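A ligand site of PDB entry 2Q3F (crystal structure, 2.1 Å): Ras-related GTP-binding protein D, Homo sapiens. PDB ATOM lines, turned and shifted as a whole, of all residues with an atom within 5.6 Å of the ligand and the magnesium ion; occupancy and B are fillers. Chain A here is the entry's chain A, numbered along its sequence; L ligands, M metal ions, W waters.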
ATOM      1  N   GLY A  11       5.956 -29.709   0.109  1.00  0.00           N
ATOM      2  CA  GLY A  11       4.752 -30.448  -0.231  1.00  0.00           C
ATOM      3  C   GLY A  11       4.882 -30.998  -1.639  1.00  0.00           C
ATOM      4  O   GLY A  11       5.878 -30.732  -2.331  1.00  0.00           O
ATOM      5  N   LEU A  12       3.888 -31.767  -2.079  1.00  0.00           N
ATOM      6  CA  LEU A  12       3.893 -32.357  -3.410  1.00  0.00           C
ATOM      7  C   LEU A  12       3.707 -31.288  -4.475  1.00  0.00           C
ATOM      8  O   LEU A  12       3.227 -30.190  -4.194  1.00  0.00           O
ATOM      9  CB  LEU A  12       2.766 -33.385  -3.531  1.00  0.00           C
ATOM     10  CG  LEU A  12       2.752 -34.568  -2.553  1.00  0.00           C
ATOM     11  CD1 LEU A  12       1.470 -35.369  -2.755  1.00  0.00           C
ATOM     12  CD2 LEU A  12       3.971 -35.456  -2.769  1.00  0.00           C
ATOM     13  N   ARG A  13       4.063 -31.601  -5.718  1.00  0.00           N
ATOM     14  CA  ARG A  13       3.891 -30.654  -6.801  1.00  0.00           C
ATOM     15  C   ARG A  13       2.435 -30.233  -6.905  1.00  0.00           C
ATOM     16  O   ARG A  13       1.526 -31.017  -6.625  1.00  0.00           O
ATOM     17  CB  ARG A  13       4.355 -31.259  -8.119  1.00  0.00           C
ATOM     18  CG  ARG A  13       5.797 -31.674  -8.058  1.00  0.00           C
ATOM     19  CD  ARG A  13       6.447 -31.843  -9.414  1.00  0.00           C
ATOM     20  NE  ARG A  13       7.893 -31.962  -9.208  1.00  0.00           N
ATOM     21  CZ  ARG A  13       8.646 -30.991  -8.688  1.00  0.00           C
ATOM     22  NH1 ARG A  13       8.103 -29.827  -8.340  1.00  0.00           N
ATOM     23  NH2 ARG A  13       9.950 -31.201  -8.489  1.00  0.00           N
ATOM     24  N   ARG A  14       2.245 -28.977  -7.299  1.00  0.00           N
ATOM     25  CA  ARG A  14       0.927 -28.382  -7.495  1.00  0.00           C
ATOM     26  C   ARG A  14       0.092 -28.173  -6.235  1.00  0.00           C
ATOM     27  O   ARG A  14      -1.085 -27.786  -6.324  1.00  0.00           O
ATOM     28  CB  ARG A  14       0.132 -29.218  -8.507  1.00  0.00           C
ATOM     29  N   SER A  15       0.666 -28.428  -5.063  1.00  0.00           N
ATOM     30  CA  SER A  15      -0.095 -28.226  -3.827  1.00  0.00           C
ATOM     31  C   SER A  15      -0.364 -26.740  -3.577  1.00  0.00           C
ATOM     32  O   SER A  15      -1.230 -26.390  -2.774  1.00  0.00           O
ATOM     33  CB  SER A  15       0.640 -28.870  -2.628  1.00  0.00           C
ATOM     34  OG  SER A  15       1.994 -28.461  -2.520  1.00  0.00           O
ATOM     35  N   GLY A  16       0.353 -25.867  -4.290  1.00  0.00           N
ATOM     36  CA  GLY A  16       0.129 -24.430  -4.156  1.00  0.00           C
ATOM     37  C   GLY A  16       1.190 -23.629  -3.420  1.00  0.00           C
ATOM     38  O   GLY A  16       0.948 -22.489  -3.018  1.00  0.00           O
ATOM     39  N   LYS A  17       2.369 -24.205  -3.257  1.00  0.00           N
ATOM     40  CA  LYS A  17       3.478 -23.556  -2.545  1.00  0.00           C
ATOM     41  C   LYS A  17       3.868 -22.189  -3.110  1.00  0.00           C
ATOM     42  O   LYS A  17       3.841 -21.187  -2.386  1.00  0.00           O
ATOM     43  CB  LYS A  17       4.697 -24.484  -2.540  1.00  0.00           C
ATOM     44  CG  LYS A  17       4.441 -25.818  -1.817  1.00  0.00           C
ATOM     45  CD  LYS A  17       5.648 -26.722  -1.838  1.00  0.00           C
ATOM     46  CE  LYS A  17       6.032 -27.137  -3.271  1.00  0.00           C
ATOM     47  NZ  LYS A  17       5.049 -28.028  -3.933  1.00  0.00           N
ATOM     48  N   SER A  18       4.224 -22.133  -4.386  1.00  0.00           N
ATOM     49  CA  SER A  18       4.634 -20.876  -5.008  1.00  0.00           C
ATOM     50  C   SER A  18       3.532 -19.822  -5.007  1.00  0.00           C
ATOM     51  O   SER A  18       3.796 -18.632  -4.829  1.00  0.00           O
ATOM     52  CB  SER A  18       5.131 -21.126  -6.423  1.00  0.00           C
ATOM     53  OG  SER A  18       6.238 -22.011  -6.419  1.00  0.00           O
ATOM     54  N   SER A  19       2.295 -20.259  -5.238  1.00  0.00           N
ATOM     55  CA  SER A  19       1.150 -19.354  -5.251  1.00  0.00           C
ATOM     56  C   SER A  19       1.088 -18.666  -3.872  1.00  0.00           C
ATOM     57  O   SER A  19       0.909 -17.459  -3.770  1.00  0.00           O
ATOM     58  CB  SER A  19      -0.147 -20.133  -5.468  1.00  0.00           C
ATOM     59  OG  SER A  19      -0.132 -20.827  -6.696  1.00  0.00           O
ATOM     60  N   ILE A  20       1.230 -19.485  -2.845  1.00  0.00           N
ATOM     61  CA  ILE A  20       1.199 -19.008  -1.470  1.00  0.00           C
ATOM     62  C   ILE A  20       2.306 -17.977  -1.234  1.00  0.00           C
ATOM     63  O   ILE A  20       2.060 -16.922  -0.660  1.00  0.00           O
ATOM     64  CB  ILE A  20       1.337 -20.198  -0.485  1.00  0.00           C
ATOM     65  CG1 ILE A  20       0.032 -20.988  -0.483  1.00  0.00           C
ATOM     66  CG2 ILE A  20       1.686 -19.701   0.904  1.00  0.00           C
ATOM     67  CD1 ILE A  20       0.129 -22.343   0.162  1.00  0.00           C
ATOM     68  N   PRO A  30      -4.318 -13.602  -6.663  1.00  0.00           N
ATOM     69  CA  PRO A  30      -4.480 -15.056  -6.715  1.00  0.00           C
ATOM     70  C   PRO A  30      -4.729 -15.519  -8.154  1.00  0.00           C
ATOM     71  O   PRO A  30      -4.292 -16.604  -8.542  1.00  0.00           O
ATOM     72  CB  PRO A  30      -5.664 -15.303  -5.775  1.00  0.00           C
ATOM     73  CG  PRO A  30      -6.424 -14.021  -5.800  1.00  0.00           C
ATOM     74  CD  PRO A  30      -5.335 -12.985  -5.799  1.00  0.00           C
ATOM     75  N   THR A  33      -1.560 -16.260 -10.190  1.00  0.00           N
ATOM     76  CA  THR A  33      -0.831 -17.484  -9.905  1.00  0.00           C
ATOM     77  C   THR A  33      -1.093 -18.564 -10.971  1.00  0.00           C
ATOM     78  O   THR A  33      -0.379 -19.565 -11.017  1.00  0.00           O
ATOM     79  CB  THR A  33      -1.190 -18.055  -8.518  1.00  0.00           C
ATOM     80  OG1 THR A  33      -2.557 -18.463  -8.490  1.00  0.00           O
ATOM     81  CG2 THR A  33      -0.954 -16.999  -7.442  1.00  0.00           C
ATOM     82  N   LEU A  34      -2.114 -18.370 -11.798  1.00  0.00           N
ATOM     83  CA  LEU A  34      -2.406 -19.342 -12.853  1.00  0.00           C
ATOM     84  C   LEU A  34      -1.289 -19.312 -13.876  1.00  0.00           C
ATOM     85  O   LEU A  34      -1.152 -20.219 -14.691  1.00  0.00           O
ATOM     86  CB  LEU A  34      -3.718 -19.005 -13.585  1.00  0.00           C
ATOM     87  CG  LEU A  34      -5.070 -19.098 -12.881  1.00  0.00           C
ATOM     88  CD1 LEU A  34      -6.145 -18.619 -13.841  1.00  0.00           C
ATOM     89  CD2 LEU A  34      -5.362 -20.517 -12.459  1.00  0.00           C
ATOM     90  N   PHE A  35      -0.481 -18.249 -13.829  1.00  0.00           N
ATOM     91  CA  PHE A  35       0.624 -18.094 -14.758  1.00  0.00           C
ATOM     92  C   PHE A  35       1.933 -18.672 -14.247  1.00  0.00           C
ATOM     93  O   PHE A  35       2.908 -18.797 -15.012  1.00  0.00           O
ATOM     94  CB  PHE A  35       0.808 -16.624 -15.123  1.00  0.00           C
ATOM     95  CG  PHE A  35      -0.340 -16.042 -15.887  1.00  0.00           C
ATOM     96  CD1 PHE A  35      -1.417 -15.446 -15.230  1.00  0.00           C
ATOM     97  CD2 PHE A  35      -0.371 -16.103 -17.277  1.00  0.00           C
ATOM     98  CE1 PHE A  35      -2.495 -14.914 -15.949  1.00  0.00           C
ATOM     99  CE2 PHE A  35      -1.444 -15.578 -18.007  1.00  0.00           C
ATOM    100  CZ  PHE A  35      -2.500 -14.988 -17.339  1.00  0.00           C
ATOM    101  N   LEU A  36       1.989 -19.018 -12.963  1.00  0.00           N
ATOM    102  CA  LEU A  36       3.198 -19.595 -12.402  1.00  0.00           C
ATOM    103  C   LEU A  36       3.459 -20.925 -13.090  1.00  0.00           C
ATOM    104  O   LEU A  36       2.518 -21.571 -13.566  1.00  0.00           O
ATOM    105  CB  LEU A  36       3.048 -19.823 -10.891  1.00  0.00           C
ATOM    106  CG  LEU A  36       2.892 -18.560 -10.052  1.00  0.00           C
ATOM    107  CD1 LEU A  36       2.482 -18.915  -8.630  1.00  0.00           C
ATOM    108  CD2 LEU A  36       4.202 -17.776 -10.066  1.00  0.00           C
ATOM    109  N   GLU A  37       4.719 -21.307 -13.170  1.00  0.00           N
ATOM    110  CA  GLU A  37       5.101 -22.576 -13.777  1.00  0.00           C
ATOM    111  C   GLU A  37       5.668 -23.454 -12.671  1.00  0.00           C
ATOM    112  O   GLU A  37       5.929 -22.969 -11.564  1.00  0.00           O
ATOM    113  CB  GLU A  37       6.162 -22.374 -14.855  1.00  0.00           C
ATOM    114  CG  GLU A  37       5.686 -21.600 -16.092  1.00  0.00           C
ATOM    115  CD  GLU A  37       4.405 -22.173 -16.695  1.00  0.00           C
ATOM    116  OE1 GLU A  37       4.353 -23.387 -16.991  1.00  0.00           O
ATOM    117  OE2 GLU A  37       3.441 -21.393 -16.866  1.00  0.00           O
ATOM    118  N   SER A  38       5.845 -24.745 -12.952  1.00  0.00           N
ATOM    119  CA  SER A  38       6.396 -25.669 -11.980  1.00  0.00           C
ATOM    120  C   SER A  38       7.751 -25.153 -11.504  1.00  0.00           C
ATOM    121  O   SER A  38       8.557 -24.665 -12.305  1.00  0.00           O
ATOM    122  CB  SER A  38       6.573 -27.050 -12.612  1.00  0.00           C
ATOM    123  OG  SER A  38       5.325 -27.556 -13.048  1.00  0.00           O
ATOM    124  N   THR A  39       8.008 -25.275 -10.201  1.00  0.00           N
ATOM    125  CA  THR A  39       9.270 -24.832  -9.602  1.00  0.00           C
ATOM    126  C   THR A  39      10.333 -25.913  -9.799  1.00  0.00           C
ATOM    127  O   THR A  39      10.127 -27.068  -9.434  1.00  0.00           O
ATOM    128  CB  THR A  39       9.124 -24.565  -8.092  1.00  0.00           C
ATOM    129  OG1 THR A  39       8.112 -23.580  -7.878  1.00  0.00           O
ATOM    130  CG2 THR A  39      10.437 -24.061  -7.519  1.00  0.00           C
ATOM    131  N   ASP A  59      10.951 -21.611  -0.950  1.00  0.00           N
ATOM    132  CA  ASP A  59       9.916 -22.266  -1.729  1.00  0.00           C
ATOM    133  C   ASP A  59      10.571 -23.439  -2.470  1.00  0.00           C
ATOM    134  O   ASP A  59      11.370 -23.224  -3.387  1.00  0.00           O
ATOM    135  CB  ASP A  59       9.313 -21.249  -2.708  1.00  0.00           C
ATOM    136  CG  ASP A  59       8.254 -21.848  -3.599  1.00  0.00           C
ATOM    137  OD1 ASP A  59       7.699 -22.901  -3.235  1.00  0.00           O
ATOM    138  OD2 ASP A  59       7.978 -21.243  -4.664  1.00  0.00           O
ATOM    139  N   PHE A  60      10.244 -24.657  -2.058  1.00  0.00           N
ATOM    140  CA  PHE A  60      10.802 -25.880  -2.648  1.00  0.00           C
ATOM    141  C   PHE A  60      10.017 -26.444  -3.810  1.00  0.00           C
ATOM    142  O   PHE A  60       8.806 -26.274  -3.893  1.00  0.00           O
ATOM    143  CB  PHE A  60      10.892 -27.008  -1.595  1.00  0.00           C
ATOM    144  CG  PHE A  60      11.972 -26.836  -0.592  1.00  0.00           C
ATOM    145  CD1 PHE A  60      11.877 -25.859   0.391  1.00  0.00           C
ATOM    146  CD2 PHE A  60      13.117 -27.635  -0.639  1.00  0.00           C
ATOM    147  CE1 PHE A  60      12.906 -25.674   1.317  1.00  0.00           C
ATOM    148  CE2 PHE A  60      14.151 -27.457   0.275  1.00  0.00           C
ATOM    149  CZ  PHE A  60      14.043 -26.473   1.259  1.00  0.00           C
ATOM    150  N   PRO A  61      10.703 -27.124  -4.741  1.00  0.00           N
ATOM    151  CA  PRO A  61       9.923 -27.696  -5.830  1.00  0.00           C
ATOM    152  C   PRO A  61       9.215 -28.911  -5.201  1.00  0.00           C
ATOM    153  O   PRO A  61       9.701 -29.444  -4.201  1.00  0.00           O
ATOM    154  CB  PRO A  61      10.988 -28.076  -6.862  1.00  0.00           C
ATOM    155  CG  PRO A  61      12.236 -28.214  -6.060  1.00  0.00           C
ATOM    156  CD  PRO A  61      12.135 -27.095  -5.071  1.00  0.00           C
ATOM    157  N   GLY A  62       8.085 -29.318  -5.770  1.00  0.00           N
ATOM    158  CA  GLY A  62       7.332 -30.439  -5.222  1.00  0.00           C
ATOM    159  C   GLY A  62       8.126 -31.706  -5.007  1.00  0.00           C
ATOM    160  O   GLY A  62       8.938 -32.089  -5.850  1.00  0.00           O
ATOM    161  N   GLN A  90      -8.153 -30.828  -2.422  1.00  0.00           N
ATOM    162  CA  GLN A  90      -9.073 -31.195  -3.492  1.00  0.00           C
ATOM    163  C   GLN A  90      -8.469 -32.303  -4.335  1.00  0.00           C
ATOM    164  O   GLN A  90      -8.839 -32.494  -5.494  1.00  0.00           O
ATOM    165  CB  GLN A  90      -9.373 -30.007  -4.393  1.00  0.00           C
ATOM    166  CG  GLN A  90     -10.081 -28.846  -3.726  1.00  0.00           C
ATOM    167  CD  GLN A  90     -10.299 -27.695  -4.693  1.00  0.00           C
ATOM    168  OE1 GLN A  90     -11.045 -27.815  -5.665  1.00  0.00           O
ATOM    169  NE2 GLN A  90      -9.640 -26.576  -4.434  1.00  0.00           N
ATOM    170  N   HIS A 121      -4.649 -26.765   2.118  1.00  0.00           N
ATOM    171  CA  HIS A 121      -4.863 -25.710   1.140  1.00  0.00           C
ATOM    172  C   HIS A 121      -5.941 -25.925   0.058  1.00  0.00           C
ATOM    173  O   HIS A 121      -6.383 -27.046  -0.194  1.00  0.00           O
ATOM    174  CB  HIS A 121      -3.492 -25.437   0.501  1.00  0.00           C
ATOM    175  CG  HIS A 121      -3.388 -24.116  -0.204  1.00  0.00           C
ATOM    176  ND1 HIS A 121      -3.621 -22.914   0.423  1.00  0.00           N
ATOM    177  CD2 HIS A 121      -3.016 -23.818  -1.480  1.00  0.00           C
ATOM    178  CE1 HIS A 121      -3.398 -21.925  -0.434  1.00  0.00           C
ATOM    179  NE2 HIS A 121      -3.026 -22.447  -1.586  1.00  0.00           N
ATOM    180  N   LYS A 122      -6.335 -24.821  -0.574  1.00  0.00           N
ATOM    181  CA  LYS A 122      -7.352 -24.852  -1.627  1.00  0.00           C
ATOM    182  C   LYS A 122      -8.731 -25.258  -1.078  1.00  0.00           C
ATOM    183  O   LYS A 122      -9.528 -25.867  -1.788  1.00  0.00           O
ATOM    184  CB  LYS A 122      -6.933 -25.826  -2.737  1.00  0.00           C
ATOM    185  CG  LYS A 122      -5.543 -25.567  -3.303  1.00  0.00           C
ATOM    186  CD  LYS A 122      -5.269 -26.446  -4.528  1.00  0.00           C
ATOM    187  CE  LYS A 122      -3.952 -26.086  -5.197  1.00  0.00           C
ATOM    188  NZ  LYS A 122      -3.643 -26.957  -6.361  1.00  0.00           N
ATOM    189  N   VAL A 123      -8.991 -24.923   0.186  1.00  0.00           N
ATOM    190  CA  VAL A 123     -10.267 -25.292   0.794  1.00  0.00           C
ATOM    191  C   VAL A 123     -11.431 -24.509   0.203  1.00  0.00           C
ATOM    192  O   VAL A 123     -12.586 -24.850   0.421  1.00  0.00           O
ATOM    193  CB  VAL A 123     -10.251 -25.080   2.339  1.00  0.00           C
ATOM    194  CG1 VAL A 123      -9.129 -25.889   2.958  1.00  0.00           C
ATOM    195  CG2 VAL A 123     -10.094 -23.596   2.667  1.00  0.00           C
ATOM    196  N   ASP A 124     -11.129 -23.468  -0.561  1.00  0.00           N
ATOM    197  CA  ASP A 124     -12.179 -22.670  -1.195  1.00  0.00           C
ATOM    198  C   ASP A 124     -13.095 -23.559  -2.039  1.00  0.00           C
ATOM    199  O   ASP A 124     -14.245 -23.210  -2.307  1.00  0.00           O
ATOM    200  CB  ASP A 124     -11.565 -21.570  -2.067  1.00  0.00           C
ATOM    201  CG  ASP A 124     -10.447 -22.082  -2.956  1.00  0.00           C
ATOM    202  OD1 ASP A 124      -9.363 -22.398  -2.429  1.00  0.00           O
ATOM    203  OD2 ASP A 124     -10.657 -22.186  -4.182  1.00  0.00           O
ATOM    204  N   GLY A 125     -12.575 -24.720  -2.431  1.00  0.00           N
ATOM    205  CA  GLY A 125     -13.363 -25.635  -3.235  1.00  0.00           C
ATOM    206  C   GLY A 125     -14.007 -26.782  -2.478  1.00  0.00           C
ATOM    207  O   GLY A 125     -14.213 -27.861  -3.036  1.00  0.00           O
ATOM    208  N   THR A 161      -6.639 -23.398   4.562  1.00  0.00           N
ATOM    209  CA  THR A 161      -6.222 -22.205   3.823  1.00  0.00           C
ATOM    210  C   THR A 161      -6.636 -22.117   2.370  1.00  0.00           C
ATOM    211  O   THR A 161      -6.899 -23.111   1.706  1.00  0.00           O
ATOM    212  CB  THR A 161      -4.682 -22.072   3.873  1.00  0.00           C
ATOM    213  OG1 THR A 161      -4.079 -23.228   3.270  1.00  0.00           O
ATOM    214  CG2 THR A 161      -4.185 -21.975   5.305  1.00  0.00           C
ATOM    215  N   SER A 162      -6.656 -20.874   1.878  1.00  0.00           N
ATOM    216  CA  SER A 162      -6.989 -20.571   0.498  1.00  0.00           C
ATOM    217  C   SER A 162      -6.371 -19.239   0.111  1.00  0.00           C
ATOM    218  O   SER A 162      -6.371 -18.301   0.902  1.00  0.00           O
ATOM    219  CB  SER A 162      -8.499 -20.493   0.301  1.00  0.00           C
ATOM    220  OG  SER A 162      -8.825 -20.142  -1.039  1.00  0.00           O
ATOM    221  N   ILE A 163      -5.823 -19.157  -1.098  1.00  0.00           N
ATOM    222  CA  ILE A 163      -5.230 -17.896  -1.545  1.00  0.00           C
ATOM    223  C   ILE A 163      -6.348 -16.946  -1.987  1.00  0.00           C
ATOM    224  O   ILE A 163      -6.095 -15.777  -2.255  1.00  0.00           O
ATOM    225  CB  ILE A 163      -4.257 -18.077  -2.745  1.00  0.00           C
ATOM    226  CG1 ILE A 163      -4.989 -18.711  -3.935  1.00  0.00           C
ATOM    227  CG2 ILE A 163      -3.046 -18.904  -2.323  1.00  0.00           C
ATOM    228  CD1 ILE A 163      -4.136 -18.812  -5.198  1.00  0.00           C
ATOM    229  N   TYR A 164      -7.576 -17.455  -2.070  1.00  0.00           N
ATOM    230  CA  TYR A 164      -8.678 -16.592  -2.497  1.00  0.00           C
ATOM    231  C   TYR A 164      -9.395 -15.834  -1.374  1.00  0.00           C
ATOM    232  O   TYR A 164     -10.444 -15.242  -1.599  1.00  0.00           O
ATOM    233  CB  TYR A 164      -9.673 -17.380  -3.338  1.00  0.00           C
ATOM    234  CG  TYR A 164      -9.118 -17.744  -4.700  1.00  0.00           C
ATOM    235  CD1 TYR A 164      -8.515 -18.985  -4.927  1.00  0.00           C
ATOM    236  CD2 TYR A 164      -9.156 -16.829  -5.755  1.00  0.00           C
ATOM    237  CE1 TYR A 164      -7.960 -19.303  -6.177  1.00  0.00           C
ATOM    238  CE2 TYR A 164      -8.609 -17.129  -6.999  1.00  0.00           C
ATOM    239  CZ  TYR A 164      -8.012 -18.367  -7.206  1.00  0.00           C
ATOM    240  OH  TYR A 164      -7.447 -18.646  -8.419  1.00  0.00           O
HETATM  241  P1  LIG L   1       5.525 -27.156  -7.875  1.00  0.00           P
HETATM  242  O1  LIG L   1       6.364 -25.943  -8.071  1.00  0.00           O
HETATM  243  O2  LIG L   1       5.451 -28.034  -9.060  1.00  0.00           O
HETATM  244  O3  LIG L   1       5.824 -27.876  -6.612  1.00  0.00           O
HETATM  245  N1  LIG L   1       3.930 -26.556  -7.670  1.00  0.00           N
HETATM  246  P2  LIG L   1       3.380 -25.554  -6.377  1.00  0.00           P
HETATM  247  O4  LIG L   1       3.344 -26.588  -5.170  1.00  0.00           O
HETATM  248  O5  LIG L   1       4.320 -24.425  -6.215  1.00  0.00           O
HETATM  249  O6  LIG L   1       1.938 -25.137  -6.874  1.00  0.00           O
HETATM  250  P3  LIG L   1       1.631 -23.745  -7.599  1.00  0.00           P
HETATM  251  O7  LIG L   1       1.888 -22.621  -6.657  1.00  0.00           O
HETATM  252  O8  LIG L   1       2.311 -23.745  -8.915  1.00  0.00           O
HETATM  253  O9  LIG L   1       0.056 -23.762  -7.753  1.00  0.00           O
HETATM  254  C1  LIG L   1      -0.637 -24.634  -8.646  1.00  0.00           C
HETATM  255  C2  LIG L   1      -1.955 -23.997  -9.030  1.00  0.00           C
HETATM  256  O10 LIG L   1      -2.898 -24.196  -7.946  1.00  0.00           O
HETATM  257  C3  LIG L   1      -1.833 -22.487  -9.156  1.00  0.00           C
HETATM  258  O11 LIG L   1      -1.508 -22.135 -10.494  1.00  0.00           O
HETATM  259  C4  LIG L   1      -3.201 -21.958  -8.763  1.00  0.00           C
HETATM  260  O12 LIG L   1      -4.033 -21.677  -9.855  1.00  0.00           O
HETATM  261  C5  LIG L   1      -3.750 -23.072  -7.866  1.00  0.00           C
HETATM  262  N2  LIG L   1      -3.943 -22.714  -6.468  1.00  0.00           N
HETATM  263  C6  LIG L   1      -2.998 -22.265  -5.570  1.00  0.00           C
HETATM  264  N3  LIG L   1      -3.512 -21.975  -4.399  1.00  0.00           N
HETATM  265  C7  LIG L   1      -4.873 -22.242  -4.545  1.00  0.00           C
HETATM  266  C8  LIG L   1      -5.955 -22.103  -3.630  1.00  0.00           C
HETATM  267  O13 LIG L   1      -5.934 -21.654  -2.471  1.00  0.00           O
HETATM  268  N4  LIG L   1      -7.152 -22.506  -4.195  1.00  0.00           N
HETATM  269  C9  LIG L   1      -7.307 -22.989  -5.468  1.00  0.00           C
HETATM  270  N5  LIG L   1      -8.535 -23.366  -5.816  1.00  0.00           N
HETATM  271  N6  LIG L   1      -6.325 -23.094  -6.332  1.00  0.00           N
HETATM  272  C10 LIG L   1      -5.140 -22.718  -5.810  1.00  0.00           C
HETATM  273 MG    MG M   1       6.129 -23.978  -7.141  1.00  0.00          MG
HETATM  274  O   HOH W   1       7.130 -24.608  -5.294  1.00  0.00           O
HETATM  275  O   HOH W   2      -0.742 -24.176 -12.691  1.00  0.00           O
HETATM  276  O   HOH W   3       5.025 -23.215  -8.977  1.00  0.00           O
HETATM  277  O   HOH W   4      -5.634 -23.323 -11.007  1.00  0.00           O
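The side-chain carboxylate of Asp 59 lies close to the side-chain hydroxyl of Ser 18, 2.6 Å away. The side-chain amino group (NZ) of Lys 17 sits at hydrogen-bond distance from the side-chain hydroxyl (OG) of Ser 15 (3.4 Å). The side-chain amino group (NZ) of Lys 17 lies within hydrogen-bond range of the backbone carbonyl oxygen (O) of Leu 12. O of Gly 11 is in hydrogen-bond range of NZ of Lys 17, at 3.3 Å. NH2 of Arg 13 sits at hydrogen-bond distance from O of Gly 62, 3.0 Å away. The backbone carbonyl oxygen (O) of Arg 14 sits at hydrogen-bond distance from the side-chain amino group (NZ) of Lys 122, 2.7 Å away. The side-chain hydroxyl of Ser 15 sits at hydrogen-bond distance from the backbone carbonyl oxygen of Leu 12 (2.7 Å). O of Lys 122 sits at hydrogen-bond distance from NE2 of Gln 90 (2.7 Å).
The magnesium ion is bound by O5 of the ligand (2.1 Å), OG of Ser 18 (2.1 Å), OG1 of Thr 39 (2.2 Å), O1 of the ligand (2.2 Å), water W1 (2.2 Å) and water W3 (2.3 Å). The magnesium ion has six donor atoms within binding distance.
Water W3 lies within hydrogen-bond range of the backbone carbonyl oxygen of Glu 37 (2.8 Å) and an oxygen (O8) of the ligand (2.8 Å). Water W1 lies within hydrogen-bond range of OD1 of Asp 59 (2.7 Å) and O of Phe 60 (2.7 Å).
Leu 12 touches the ligand (O to O4, 3.7 Å). Leu 34 touches the ligand. Ser 38 touches the ligand. Pro 61 touches the ligand. NE2 of Gln 90 touches N5 of the ligand, 3.7 Å away. Ser 162 touches the ligand. CE1 of Tyr 164 touches C9 of the ligand (3.8 Å). Hydrophobic or aromatic side chains that line the ligand: Leu 34, His 121, Ile 163 and Tyr 164.
Within 4 Å of the magnesium ion: Ser 18 and Thr 39. The nearest printed residue that does not touch the magnesium ion is Asp 59 (4.1 Å).
An oxygen (O7) of the ligand sits at hydrogen-bond distance from the backbone NH (N) of Ser 18, 3.3 Å away. N of Thr 39 sits close to O1 of the ligand. An oxygen (O4) of the ligand is in hydrogen-bond range of the backbone NH of Lys 17, 3.2 Å away. O4 of the ligand is in salt-bridge range of NZ of Lys 17 (2.6 Å). The backbone NH (N) of Ser 19 sits at hydrogen-bond distance from an oxygen (O7) of the ligand (2.8 Å). An oxygen (O7) of the ligand is in hydrogen-bond range of the side-chain hydroxyl of Ser 19 (2.7 Å). The backbone NH of Gly 62 sits at hydrogen-bond distance from an oxygen (O3) of the ligand, 2.8 Å away. The side-chain carboxylate (OD1) of Asp 124 sits at hydrogen-bond distance from a nitrogen (N4) of the ligand (2.8 Å). An oxygen (O13) of the ligand sits at hydrogen-bond distance from the backbone NH (N) of Ile 163 (2.9 Å). O of Thr 33 sits at hydrogen-bond distance from O11 of the ligand, 2.9 Å away. A ring nitrogen (NE2) of His 121 is in hydrogen-bond range of a nitrogen (N3) of the ligand, at 2.9 Å. The backbone NH (N) of Arg 14 sits at hydrogen-bond distance from an oxygen (O4) of the ligand (3.4 Å). An oxygen (O6) of the ligand lies within hydrogen-bond range of the backbone NH of Gly 16 (3.1 Å). O4 of the ligand sits at hydrogen-bond distance from N of Ser 15 (3.3 Å). The side-chain amino group (NZ) of Lys 122 is in hydrogen-bond range of an oxygen (O10) of the ligand (3.3 Å). An oxygen (O2) of the ligand lies within salt-bridge range of the guanidinium group of Arg 13.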
